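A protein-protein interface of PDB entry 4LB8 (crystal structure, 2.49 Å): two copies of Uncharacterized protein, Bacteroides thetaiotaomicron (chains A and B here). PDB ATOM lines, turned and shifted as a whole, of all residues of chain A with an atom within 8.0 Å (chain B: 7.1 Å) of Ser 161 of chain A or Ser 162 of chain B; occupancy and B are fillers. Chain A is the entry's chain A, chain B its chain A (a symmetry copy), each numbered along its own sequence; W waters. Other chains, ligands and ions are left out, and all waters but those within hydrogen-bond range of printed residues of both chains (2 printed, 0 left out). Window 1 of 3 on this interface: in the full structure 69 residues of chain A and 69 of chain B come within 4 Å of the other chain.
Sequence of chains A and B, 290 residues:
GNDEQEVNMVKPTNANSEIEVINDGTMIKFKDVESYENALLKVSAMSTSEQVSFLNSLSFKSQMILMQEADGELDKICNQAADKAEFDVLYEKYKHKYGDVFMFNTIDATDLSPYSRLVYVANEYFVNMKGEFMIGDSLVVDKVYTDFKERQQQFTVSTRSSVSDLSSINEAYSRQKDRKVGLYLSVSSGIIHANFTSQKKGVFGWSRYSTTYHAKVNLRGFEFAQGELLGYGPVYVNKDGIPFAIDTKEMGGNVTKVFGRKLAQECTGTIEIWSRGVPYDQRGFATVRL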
ATOM      1  N   SER A 158     -30.053 -17.991   1.650  1.00  0.00           N
ATOM      2  CA  SER A 158     -29.136 -18.635   0.718  1.00  0.00           C
ATOM      3  C   SER A 158     -28.369 -19.790   1.347  1.00  0.00           C
ATOM      4  O   SER A 158     -27.952 -19.727   2.502  1.00  0.00           O
ATOM      5  CB  SER A 158     -28.155 -17.627   0.120  1.00  0.00           C
ATOM      6  OG  SER A 158     -26.960 -17.461   0.865  1.00  0.00           O
ATOM      7  N   THR A 159     -28.190 -20.840   0.544  1.00  0.00           N
ATOM      8  CA  THR A 159     -27.431 -22.030   0.873  1.00  0.00           C
ATOM      9  C   THR A 159     -26.412 -22.280  -0.257  1.00  0.00           C
ATOM     10  O   THR A 159     -26.535 -21.711  -1.350  1.00  0.00           O
ATOM     11  CB  THR A 159     -28.361 -23.242   1.108  1.00  0.00           C
ATOM     12  OG1 THR A 159     -29.165 -23.476  -0.043  1.00  0.00           O
ATOM     13  CG2 THR A 159     -29.250 -23.092   2.323  1.00  0.00           C
ATOM     14  N   ARG A 160     -25.397 -23.109   0.026  1.00  0.00           N
ATOM     15  CA  ARG A 160     -24.401 -23.553  -0.957  1.00  0.00           C
ATOM     16  C   ARG A 160     -25.036 -24.574  -1.886  1.00  0.00           C
ATOM     17  O   ARG A 160     -24.759 -24.618  -3.074  1.00  0.00           O
ATOM     18  CB  ARG A 160     -23.217 -24.202  -0.221  1.00  0.00           C
ATOM     19  CG  ARG A 160     -22.052 -24.521  -1.114  1.00  0.00           C
ATOM     20  CD  ARG A 160     -20.931 -25.040  -0.285  1.00  0.00           C
ATOM     21  NE  ARG A 160     -19.930 -25.743  -1.080  1.00  0.00           N
ATOM     22  CZ  ARG A 160     -18.913 -25.161  -1.702  1.00  0.00           C
ATOM     23  NH1 ARG A 160     -18.756 -23.845  -1.644  1.00  0.00           N
ATOM     24  NH2 ARG A 160     -18.043 -25.892  -2.383  1.00  0.00           N
ATOM     25  N   SER A 161     -25.871 -25.429  -1.306  1.00  0.00           N
ATOM     26  CA  SER A 161     -26.512 -26.526  -2.000  1.00  0.00           C
ATOM     27  C   SER A 161     -27.924 -26.757  -1.460  1.00  0.00           C
ATOM     28  O   SER A 161     -28.119 -26.634  -0.244  1.00  0.00           O
ATOM     29  CB  SER A 161     -25.662 -27.781  -1.834  1.00  0.00           C
ATOM     30  OG  SER A 161     -26.061 -28.757  -2.780  1.00  0.00           O
ATOM     31  N   SER A 162     -28.903 -27.077  -2.373  1.00  0.00           N
ATOM     32  CA  SER A 162     -30.315 -27.417  -2.100  1.00  0.00           C
ATOM     33  C   SER A 162     -30.838 -28.358  -3.173  1.00  0.00           C
ATOM     34  O   SER A 162     -30.700 -28.086  -4.376  1.00  0.00           O
ATOM     35  CB  SER A 162     -31.208 -26.187  -2.021  1.00  0.00           C
ATOM     36  OG  SER A 162     -30.999 -25.525  -0.787  1.00  0.00           O
ATOM     37  N   VAL A 163     -31.418 -29.477  -2.728  1.00  0.00           N
ATOM     38  CA  VAL A 163     -31.938 -30.530  -3.579  1.00  0.00           C
ATOM     39  C   VAL A 163     -33.345 -30.833  -3.079  1.00  0.00           C
ATOM     40  O   VAL A 163     -33.531 -30.980  -1.865  1.00  0.00           O
ATOM     41  CB  VAL A 163     -30.996 -31.767  -3.571  1.00  0.00           C
ATOM     42  CG1 VAL A 163     -31.527 -32.899  -4.441  1.00  0.00           C
ATOM     43  CG2 VAL A 163     -29.582 -31.388  -3.993  1.00  0.00           C
ATOM     44  N   SER A 164     -34.345 -30.846  -3.994  1.00  0.00           N
ATOM     45  CA  SER A 164     -35.741 -31.063  -3.629  1.00  0.00           C
ATOM     46  C   SER A 164     -36.003 -32.519  -3.289  1.00  0.00           C
ATOM     47  O   SER A 164     -35.342 -33.395  -3.842  1.00  0.00           O
ATOM     48  CB  SER A 164     -36.665 -30.616  -4.756  1.00  0.00           C
ATOM     49  OG  SER A 164     -36.511 -31.365  -5.955  1.00  0.00           O
ATOM     50  N   TYR A 173     -35.640 -30.020  -8.417  1.00  0.00           N
ATOM     51  CA  TYR A 173     -34.448 -29.227  -8.646  1.00  0.00           C
ATOM     52  C   TYR A 173     -33.262 -29.778  -7.891  1.00  0.00           C
ATOM     53  O   TYR A 173     -33.404 -30.550  -6.942  1.00  0.00           O
ATOM     54  CB  TYR A 173     -34.680 -27.730  -8.267  1.00  0.00           C
ATOM     55  CG  TYR A 173     -35.043 -27.494  -6.812  1.00  0.00           C
ATOM     56  CD1 TYR A 173     -34.054 -27.379  -5.832  1.00  0.00           C
ATOM     57  CD2 TYR A 173     -36.376 -27.389  -6.410  1.00  0.00           C
ATOM     58  CE1 TYR A 173     -34.382 -27.203  -4.485  1.00  0.00           C
ATOM     59  CE2 TYR A 173     -36.716 -27.186  -5.065  1.00  0.00           C
ATOM     60  CZ  TYR A 173     -35.715 -27.109  -4.103  1.00  0.00           C
ATOM     61  OH  TYR A 173     -36.048 -26.944  -2.771  1.00  0.00           O
ATOM     62  N   SER A 174     -32.075 -29.305  -8.289  1.00  0.00           N
ATOM     63  CA  SER A 174     -30.817 -29.549  -7.628  1.00  0.00           C
ATOM     64  C   SER A 174     -29.924 -28.355  -7.885  1.00  0.00           C
ATOM     65  O   SER A 174     -29.544 -28.115  -9.027  1.00  0.00           O
ATOM     66  CB  SER A 174     -30.191 -30.849  -8.092  1.00  0.00           C
ATOM     67  OG  SER A 174     -29.137 -31.214  -7.219  1.00  0.00           O
ATOM     68  N   ARG A 175     -29.727 -27.509  -6.862  1.00  0.00           N
ATOM     69  CA  ARG A 175     -28.835 -26.359  -6.998  1.00  0.00           C
ATOM     70  C   ARG A 175     -27.550 -26.693  -6.280  1.00  0.00           C
ATOM     71  O   ARG A 175     -27.554 -26.906  -5.074  1.00  0.00           O
ATOM     72  CB  ARG A 175     -29.439 -25.049  -6.482  1.00  0.00           C
ATOM     73  CG  ARG A 175     -28.448 -23.872  -6.622  1.00  0.00           C
ATOM     74  CD  ARG A 175     -28.930 -22.575  -5.999  1.00  0.00           C
ATOM     75  NE  ARG A 175     -28.473 -22.492  -4.616  1.00  0.00           N
ATOM     76  CZ  ARG A 175     -29.254 -22.676  -3.563  1.00  0.00           C
ATOM     77  NH1 ARG A 175     -30.553 -22.900  -3.722  1.00  0.00           N
ATOM     78  NH2 ARG A 175     -28.755 -22.605  -2.345  1.00  0.00           N
ATOM     79  N   GLN A 176     -26.469 -26.790  -7.020  1.00  0.00           N
ATOM     80  CA  GLN A 176     -25.192 -27.124  -6.422  1.00  0.00           C
ATOM     81  C   GLN A 176     -24.336 -25.851  -6.305  1.00  0.00           C
ATOM     82  O   GLN A 176     -24.860 -24.757  -6.439  1.00  0.00           O
ATOM     83  CB  GLN A 176     -24.516 -28.266  -7.216  1.00  0.00           C
ATOM     84  CG  GLN A 176     -25.294 -29.592  -7.142  1.00  0.00           C
ATOM     85  CD  GLN A 176     -25.441 -30.129  -5.725  1.00  0.00           C
ATOM     86  OE1 GLN A 176     -26.552 -30.388  -5.261  1.00  0.00           O
ATOM     87  NE2 GLN A 176     -24.326 -30.283  -4.989  1.00  0.00           N
ATOM     88  N   LYS A 177     -23.049 -25.985  -5.997  1.00  0.00           N
ATOM     89  CA  LYS A 177     -22.186 -24.837  -5.759  1.00  0.00           C
ATOM     90  C   LYS A 177     -22.030 -23.912  -7.003  1.00  0.00           C
ATOM     91  O   LYS A 177     -21.984 -22.695  -6.832  1.00  0.00           O
ATOM     92  CB  LYS A 177     -20.820 -25.288  -5.185  1.00  0.00           C
ATOM     93  CG  LYS A 177     -19.808 -25.823  -6.164  1.00  0.00           C
ATOM     94  CD  LYS A 177     -18.475 -25.107  -5.994  1.00  0.00           C
ATOM     95  CE  LYS A 177     -17.544 -25.329  -7.162  1.00  0.00           C
ATOM     96  NZ  LYS A 177     -17.064 -26.732  -7.228  1.00  0.00           N
ATOM     97  N   ASP A 178     -21.969 -24.470  -8.226  1.00  0.00           N
ATOM     98  CA  ASP A 178     -21.810 -23.639  -9.414  1.00  0.00           C
ATOM     99  C   ASP A 178     -22.618 -24.155 -10.617  1.00  0.00           C
ATOM    100  O   ASP A 178     -22.489 -23.597 -11.707  1.00  0.00           O
ATOM    101  CB  ASP A 178     -20.328 -23.429  -9.768  1.00  0.00           C
ATOM    102  CG  ASP A 178     -19.533 -24.655 -10.163  1.00  0.00           C
ATOM    103  OD1 ASP A 178     -20.137 -25.738 -10.305  1.00  0.00           O
ATOM    104  OD2 ASP A 178     -18.310 -24.521 -10.370  1.00  0.00           O
ATOM    105  N   ARG A 179     -23.512 -25.157 -10.390  1.00  0.00           N
ATOM    106  CA  ARG A 179     -24.441 -25.721 -11.373  1.00  0.00           C
ATOM    107  C   ARG A 179     -25.844 -25.938 -10.748  1.00  0.00           C
ATOM    108  O   ARG A 179     -25.930 -26.370  -9.602  1.00  0.00           O
ATOM    109  CB  ARG A 179     -23.915 -27.052 -11.942  1.00  0.00           C
ATOM    110  CG  ARG A 179     -22.568 -27.012 -12.663  1.00  0.00           C
ATOM    111  CD  ARG A 179     -22.591 -26.231 -13.959  1.00  0.00           C
ATOM    112  NE  ARG A 179     -21.279 -26.198 -14.607  1.00  0.00           N
ATOM    113  CZ  ARG A 179     -20.345 -25.277 -14.378  1.00  0.00           C
ATOM    114  NH1 ARG A 179     -20.564 -24.300 -13.504  1.00  0.00           N
ATOM    115  NH2 ARG A 179     -19.181 -25.332 -15.007  1.00  0.00           N
ATOM    116  N   VAL A 278     -24.729 -31.698 -12.860  1.00  0.00           N
ATOM    117  CA  VAL A 278     -25.276 -32.113 -11.558  1.00  0.00           C
ATOM    118  C   VAL A 278     -25.296 -33.646 -11.532  1.00  0.00           C
ATOM    119  O   VAL A 278     -26.031 -34.247 -12.291  1.00  0.00           O
ATOM    120  CB  VAL A 278     -26.643 -31.458 -11.196  1.00  0.00           C
ATOM    121  CG1 VAL A 278     -27.135 -31.934  -9.842  1.00  0.00           C
ATOM    122  CG2 VAL A 278     -26.535 -29.936 -11.184  1.00  0.00           C
ATOM    123  N   GLN A 282     -26.698 -36.408  -6.669  1.00  0.00           N
ATOM    124  CA  GLN A 282     -27.274 -35.149  -6.238  1.00  0.00           C
ATOM    125  C   GLN A 282     -28.574 -34.802  -7.000  1.00  0.00           C
ATOM    126  O   GLN A 282     -29.055 -33.659  -6.903  1.00  0.00           O
ATOM    127  CB  GLN A 282     -26.222 -34.039  -6.384  1.00  0.00           C
ATOM    128  CG  GLN A 282     -25.127 -34.077  -5.297  1.00  0.00           C
ATOM    129  CD  GLN A 282     -25.673 -34.054  -3.872  1.00  0.00           C
ATOM    130  OE1 GLN A 282     -25.398 -34.933  -3.049  1.00  0.00           O
ATOM    131  NE2 GLN A 282     -26.466 -33.060  -3.542  1.00  0.00           N
ATOM    132  N   VAL B 157     -41.031 -27.104   3.599  1.00  0.00           N
ATOM    133  CA  VAL B 157     -39.877 -26.455   4.224  1.00  0.00           C
ATOM    134  C   VAL B 157     -38.706 -27.437   4.082  1.00  0.00           C
ATOM    135  O   VAL B 157     -37.539 -27.025   4.021  1.00  0.00           O
ATOM    136  CB  VAL B 157     -40.187 -26.110   5.719  1.00  0.00           C
ATOM    137  CG1 VAL B 157     -38.997 -25.425   6.406  1.00  0.00           C
ATOM    138  CG2 VAL B 157     -41.457 -25.260   5.853  1.00  0.00           C
ATOM    139  N   SER B 158     -39.052 -28.749   4.014  1.00  0.00           N
ATOM    140  CA  SER B 158     -38.127 -29.872   3.919  1.00  0.00           C
ATOM    141  C   SER B 158     -37.529 -30.027   2.527  1.00  0.00           C
ATOM    142  O   SER B 158     -38.203 -29.842   1.517  1.00  0.00           O
ATOM    143  CB  SER B 158     -38.796 -31.179   4.342  1.00  0.00           C
ATOM    144  OG  SER B 158     -39.436 -31.878   3.287  1.00  0.00           O
ATOM    145  N   THR B 159     -36.243 -30.382   2.513  1.00  0.00           N
ATOM    146  CA  THR B 159     -35.463 -30.668   1.326  1.00  0.00           C
ATOM    147  C   THR B 159     -34.789 -32.042   1.510  1.00  0.00           C
ATOM    148  O   THR B 159     -34.718 -32.561   2.633  1.00  0.00           O
ATOM    149  CB  THR B 159     -34.442 -29.542   1.040  1.00  0.00           C
ATOM    150  OG1 THR B 159     -33.582 -29.362   2.159  1.00  0.00           O
ATOM    151  CG2 THR B 159     -35.087 -28.222   0.681  1.00  0.00           C
ATOM    152  N   ARG B 160     -34.323 -32.634   0.402  1.00  0.00           N
ATOM    153  CA  ARG B 160     -33.552 -33.884   0.399  1.00  0.00           C
ATOM    154  C   ARG B 160     -32.144 -33.604   0.896  1.00  0.00           C
ATOM    155  O   ARG B 160     -31.541 -34.404   1.593  1.00  0.00           O
ATOM    156  CB  ARG B 160     -33.485 -34.434  -1.036  1.00  0.00           C
ATOM    157  CG  ARG B 160     -32.885 -35.808  -1.128  1.00  0.00           C
ATOM    158  CD  ARG B 160     -32.970 -36.283  -2.535  1.00  0.00           C
ATOM    159  NE  ARG B 160     -32.071 -37.402  -2.800  1.00  0.00           N
ATOM    160  CZ  ARG B 160     -32.366 -38.676  -2.581  1.00  0.00           C
ATOM    161  NH1 ARG B 160     -33.542 -39.015  -2.070  1.00  0.00           N
ATOM    162  NH2 ARG B 160     -31.487 -39.623  -2.876  1.00  0.00           N
ATOM    163  N   SER B 161     -31.612 -32.458   0.486  1.00  0.00           N
ATOM    164  CA  SER B 161     -30.256 -32.048   0.780  1.00  0.00           C
ATOM    165  C   SER B 161     -30.181 -30.534   0.987  1.00  0.00           C
ATOM    166  O   SER B 161     -30.875 -29.804   0.266  1.00  0.00           O
ATOM    167  CB  SER B 161     -29.348 -32.478  -0.366  1.00  0.00           C
ATOM    168  OG  SER B 161     -27.995 -32.417   0.047  1.00  0.00           O
ATOM    169  N   SER B 162     -29.348 -30.074   1.981  1.00  0.00           N
ATOM    170  CA  SER B 162     -29.046 -28.669   2.327  1.00  0.00           C
ATOM    171  C   SER B 162     -27.646 -28.570   2.911  1.00  0.00           C
ATOM    172  O   SER B 162     -27.293 -29.313   3.839  1.00  0.00           O
ATOM    173  CB  SER B 162     -30.050 -28.080   3.307  1.00  0.00           C
ATOM    174  OG  SER B 162     -31.258 -27.783   2.631  1.00  0.00           O
ATOM    175  N   VAL B 163     -26.846 -27.661   2.344  1.00  0.00           N
ATOM    176  CA  VAL B 163     -25.461 -27.437   2.712  1.00  0.00           C
ATOM    177  C   VAL B 163     -25.305 -25.935   2.909  1.00  0.00           C
ATOM    178  O   VAL B 163     -25.767 -25.167   2.058  1.00  0.00           O
ATOM    179  CB  VAL B 163     -24.500 -28.026   1.641  1.00  0.00           C
ATOM    180  CG1 VAL B 163     -23.036 -27.788   1.991  1.00  0.00           C
ATOM    181  CG2 VAL B 163     -24.761 -29.511   1.420  1.00  0.00           C
ATOM    182  N   SER B 164     -24.732 -25.512   4.063  1.00  0.00           N
ATOM    183  CA  SER B 164     -24.584 -24.099   4.395  1.00  0.00           C
ATOM    184  C   SER B 164     -23.475 -23.454   3.582  1.00  0.00           C
ATOM    185  O   SER B 164     -22.514 -24.135   3.229  1.00  0.00           O
ATOM    186  CB  SER B 164     -24.309 -23.923   5.884  1.00  0.00           C
ATOM    187  OG  SER B 164     -23.081 -24.499   6.311  1.00  0.00           O
ATOM    188  N   ASP B 165     -23.602 -22.145   3.289  1.00  0.00           N
ATOM    189  CA  ASP B 165     -22.573 -21.387   2.562  1.00  0.00           C
ATOM    190  C   ASP B 165     -21.941 -20.349   3.489  1.00  0.00           C
ATOM    191  O   ASP B 165     -22.392 -20.202   4.619  1.00  0.00           O
ATOM    192  CB  ASP B 165     -23.148 -20.728   1.289  1.00  0.00           C
ATOM    193  CG  ASP B 165     -24.248 -19.697   1.461  1.00  0.00           C
ATOM    194  OD1 ASP B 165     -24.578 -19.355   2.633  1.00  0.00           O
ATOM    195  OD2 ASP B 165     -24.796 -19.246   0.432  1.00  0.00           O
ATOM    196  N   TYR B 173     -23.097 -26.665   8.296  1.00  0.00           N
ATOM    197  CA  TYR B 173     -23.787 -27.939   8.245  1.00  0.00           C
ATOM    198  C   TYR B 173     -23.814 -28.499   6.843  1.00  0.00           C
ATOM    199  O   TYR B 173     -23.610 -27.787   5.860  1.00  0.00           O
ATOM    200  CB  TYR B 173     -25.239 -27.821   8.806  1.00  0.00           C
ATOM    201  CG  TYR B 173     -26.132 -26.852   8.052  1.00  0.00           C
ATOM    202  CD1 TYR B 173     -26.824 -27.252   6.906  1.00  0.00           C
ATOM    203  CD2 TYR B 173     -26.286 -25.531   8.479  1.00  0.00           C
ATOM    204  CE1 TYR B 173     -27.615 -26.355   6.184  1.00  0.00           C
ATOM    205  CE2 TYR B 173     -27.098 -24.629   7.778  1.00  0.00           C
ATOM    206  CZ  TYR B 173     -27.749 -25.042   6.620  1.00  0.00           C
ATOM    207  OH  TYR B 173     -28.523 -24.146   5.906  1.00  0.00           O
ATOM    208  N   SER B 174     -24.145 -29.794   6.764  1.00  0.00           N
ATOM    209  CA  SER B 174     -24.396 -30.516   5.540  1.00  0.00           C
ATOM    210  C   SER B 174     -25.386 -31.616   5.852  1.00  0.00           C
ATOM    211  O   SER B 174     -25.061 -32.532   6.600  1.00  0.00           O
ATOM    212  CB  SER B 174     -23.111 -31.048   4.939  1.00  0.00           C
ATOM    213  OG  SER B 174     -23.343 -31.471   3.606  1.00  0.00           O
ATOM    214  N   ARG B 175     -26.646 -31.444   5.422  1.00  0.00           N
ATOM    215  CA  ARG B 175     -27.658 -32.477   5.625  1.00  0.00           C
ATOM    216  C   ARG B 175     -27.863 -33.178   4.305  1.00  0.00           C
ATOM    217  O   ARG B 175     -28.284 -32.559   3.335  1.00  0.00           O
ATOM    218  CB  ARG B 175     -28.980 -31.940   6.184  1.00  0.00           C
ATOM    219  CG  ARG B 175     -30.025 -33.065   6.354  1.00  0.00           C
ATOM    220  CD  ARG B 175     -31.402 -32.581   6.768  1.00  0.00           C
ATOM    221  NE  ARG B 175     -32.213 -32.324   5.582  1.00  0.00           N
ATOM    222  CZ  ARG B 175     -32.500 -31.116   5.126  1.00  0.00           C
ATOM    223  NH1 ARG B 175     -32.093 -30.035   5.783  1.00  0.00           N
ATOM    224  NH2 ARG B 175     -33.222 -30.972   4.033  1.00  0.00           N
ATOM    225  N   GLN B 176     -27.523 -34.446   4.251  1.00  0.00           N
ATOM    226  CA  GLN B 176     -27.667 -35.198   3.021  1.00  0.00           C
ATOM    227  C   GLN B 176     -28.909 -36.102   3.119  1.00  0.00           C
ATOM    228  O   GLN B 176     -29.728 -35.908   4.003  1.00  0.00           O
ATOM    229  CB  GLN B 176     -26.358 -35.961   2.708  1.00  0.00           C
ATOM    230  CG  GLN B 176     -25.174 -35.023   2.407  1.00  0.00           C
ATOM    231  CD  GLN B 176     -25.406 -34.123   1.201  1.00  0.00           C
ATOM    232  OE1 GLN B 176     -25.300 -32.900   1.299  1.00  0.00           O
ATOM    233  NE2 GLN B 176     -25.758 -34.702   0.039  1.00  0.00           N
ATOM    234  N   LYS B 177     -29.080 -37.037   2.189  1.00  0.00           N
ATOM    235  CA  LYS B 177     -30.276 -37.866   2.136  1.00  0.00           C
ATOM    236  C   LYS B 177     -30.465 -38.759   3.399  1.00  0.00           C
ATOM    237  O   LYS B 177     -31.602 -38.930   3.837  1.00  0.00           O
ATOM    238  CB  LYS B 177     -30.317 -38.685   0.824  1.00  0.00           C
ATOM    239  CG  LYS B 177     -29.472 -39.931   0.766  1.00  0.00           C
ATOM    240  CD  LYS B 177     -30.311 -41.122   0.320  1.00  0.00           C
ATOM    241  CE  LYS B 177     -29.632 -42.443   0.590  1.00  0.00           C
ATOM    242  NZ  LYS B 177     -28.443 -42.642  -0.276  1.00  0.00           N
ATOM    243  N   VAL B 181     -24.202 -33.550   9.215  1.00  0.00           N
ATOM    244  CA  VAL B 181     -23.024 -33.150   9.985  1.00  0.00           C
ATOM    245  C   VAL B 181     -23.090 -31.624  10.254  1.00  0.00           C
ATOM    246  O   VAL B 181     -23.554 -30.860   9.421  1.00  0.00           O
ATOM    247  CB  VAL B 181     -21.678 -33.624   9.357  1.00  0.00           C
ATOM    248  CG1 VAL B 181     -21.362 -32.906   8.054  1.00  0.00           C
ATOM    249  CG2 VAL B 181     -20.522 -33.526  10.358  1.00  0.00           C
ATOM    250  N   GLN B 282     -19.405 -32.393  -0.502  1.00  0.00           N
ATOM    251  CA  GLN B 282     -20.644 -31.912   0.081  1.00  0.00           C
ATOM    252  C   GLN B 282     -20.426 -31.221   1.446  1.00  0.00           C
ATOM    253  O   GLN B 282     -21.408 -30.962   2.165  1.00  0.00           O
ATOM    254  CB  GLN B 282     -21.634 -33.081   0.191  1.00  0.00           C
ATOM    255  CG  GLN B 282     -22.259 -33.495  -1.158  1.00  0.00           C
ATOM    256  CD  GLN B 282     -22.935 -32.345  -1.901  1.00  0.00           C
ATOM    257  OE1 GLN B 282     -22.619 -32.033  -3.053  1.00  0.00           O
ATOM    258  NE2 GLN B 282     -23.872 -31.680  -1.266  1.00  0.00           N
ATOM    259  N   GLY B 284     -20.074 -28.560   4.377  1.00  0.00           N
ATOM    260  CA  GLY B 284     -20.740 -27.327   4.773  1.00  0.00           C
ATOM    261  C   GLY B 284     -19.757 -26.251   5.170  1.00  0.00           C
ATOM    262  O   GLY B 284     -18.733 -26.546   5.774  1.00  0.00           O
HETATM  263  O   HOH W   1     -26.689 -30.912  -1.555  1.00  0.00           O
HETATM  264  O   HOH W   2     -24.622 -19.341  -2.279  1.00  0.00           O
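The backbone NH (N) of Arg 160 of chain B lies within hydrogen-bond range of the backbone carbonyl oxygen (O) of Val 163 of chain A. OG of Ser 158 of chain A sits at hydrogen-bond distance from OD2 of Asp 165 of chain B (2.8 Å). The backbone carbonyl oxygen (O) of Ser 161 of chain A is in hydrogen-bond range of the backbone NH (N) of Val 163 of chain B (3.1 Å). N of Val 163 of chain A is in hydrogen-bond range of O of Ser 161 of chain B, at 3.1 Å. The backbone NH (N) of Arg 160 of chain A lies within hydrogen-bond range of the backbone carbonyl oxygen (O) of Val 163 of chain B (2.9 Å). The side-chain amide nitrogen of Gln 176 of chain A is in hydrogen-bond range of the side-chain amide oxygen of Gln 282 of chain B (3.1 Å). OE1 of Gln 282 of chain A lies within hydrogen-bond range of NE2 of Gln 176 of chain B (3.1 Å).
O of Ser 162 of chain B sits at hydrogen-bond distance from N of Arg 175 of chain B. The side-chain amide nitrogen (NE2) of Gln 282 of chain A lies within hydrogen-bond range of the side-chain amide oxygen (OE1) of Gln 176 of chain A. The side-chain amide oxygen (OE1) of Gln 176 of chain B is in hydrogen-bond range of the side-chain amide nitrogen (NE2) of Gln 282 of chain B. The side-chain hydroxyl of Ser 161 of chain A lies close to the backbone carbonyl oxygen of Arg 175 of chain A (3.3 Å). OE1 of Gln 176 of chain B lies within hydrogen-bond range of OG of Ser 174 of chain B. The side-chain amide oxygen (OE1) of Gln 176 of chain B is in hydrogen-bond range of the side-chain hydroxyl (OG) of Ser 161 of chain B, at 3.0 Å.
Among the printed residues, pairs that only touch across the chains: Thr 159 of chain A with Val 163 of chain B, Thr 159 of chain A with Asp 165 of chain B, Thr 159 of chain A with Tyr 173 of chain B, Arg 160 of chain A with Ser 164 of chain B, Arg 160 of chain A with Asp 165 of chain B, Ser 161 of chain A with Ser 162 of chain B, Ser 161 of chain A with Gln 282 of chain B, Ser 162 of chain A with Ser 161 of chain B, Val 163 of chain A with Thr 159 of chain B, Ser 164 of chain A with Arg 160 of chain B, Tyr 173 of chain A with Thr 159 of chain B, Gln 282 of chain A with Ser 161 of chain B and Gln 282 of chain A with Gln 282 of chain B.
Of the printed residues of chain B, Arg 160 of chain A touches Val 163 (2.9 Å), Ser 164 (3.5 Å) and Asp 165 (3.5 Å). Ser 161 of chain A touches three residues of chain B. Printed residues of chain B within 4 Å of Ser 162 of chain A: Ser 161. Printed residues of chain B within 4 Å of Gln 282 of chain A: Ser 161 (3.95 Å), Gln 176 (3.1 Å) and Gln 282 (3.7 Å). Ser 161 of chain B touches three residues of chain A. Ser 162 of chain B touches just one residue of chain A: Ser 161 (3.4 Å). Of the printed residues of chain A, Val 163 of chain B touches Thr 159, Arg 160 and Ser 161. Ser 174 of chain B touches none of the printed residues of chain A. Printed residues of chain A within 4 Å of Gln 282 of chain B: Ser 161, Gln 176 and Gln 282.
Hydrophobic or aromatic side chains of chain A that line the printed part of chain B: Val 163 and Tyr 173. Of the 17 printed residues of chain B, 10 touch a printed residue of chain A. Printed residues of chain B that touch a printed residue of chain A: Thr 159, Arg 160, Ser 161, Ser 162, Val 163, Ser 164, Asp 165, Tyr 173, Gln 176 and Gln 282. Hydrophobic or aromatic side chains of chain B within 4 Å of the printed part of chain A: Val 163 and Tyr 173. Along chain B the printed residues that touch a printed residue of chain A span positions 159 to 282.
Arg 160 of chain A touches Val 163 of chain B, and with the chains exchanged Val 163 of chain A touches Arg 160 of chain B. Ser 161 of chain A touches Ser 162 of chain B, and with the chains exchanged Ser 162 of chain A touches Ser 161 of chain B. Ser 161 of chain A touches Val 163 of chain B, and with the chains exchanged Val 163 of chain A touches Ser 161 of chain B. Gln 176 of chain A touches Gln 282 of chain B, and with the chains exchanged Gln 282 of chain A touches Gln 176 of chain B. Positions printed for both chains: 158, 159, 160, 161, 162, 163, 164, 173, 174, 175, 176, 177 and 282. Of the 20 pairs that touch across the chains among the printed residues, 17 have their exchanged pair printed and touching as well.
Water W1 lies within hydrogen-bond range of the side-chain hydroxyl (OG) of Ser 161 of chain B, the side-chain hydroxyl (OG) of Ser 161 of chain A, the side-chain amide nitrogen (NE2) of Gln 282 of chain B and the side-chain amide nitrogen (NE2) of Gln 282 of chain A. Water W2 bridges the side-chain carboxylate of Asp 165 of chain B (2.7 Å) and the backbone carbonyl oxygen of Thr 159 of chain A (3.2 Å).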
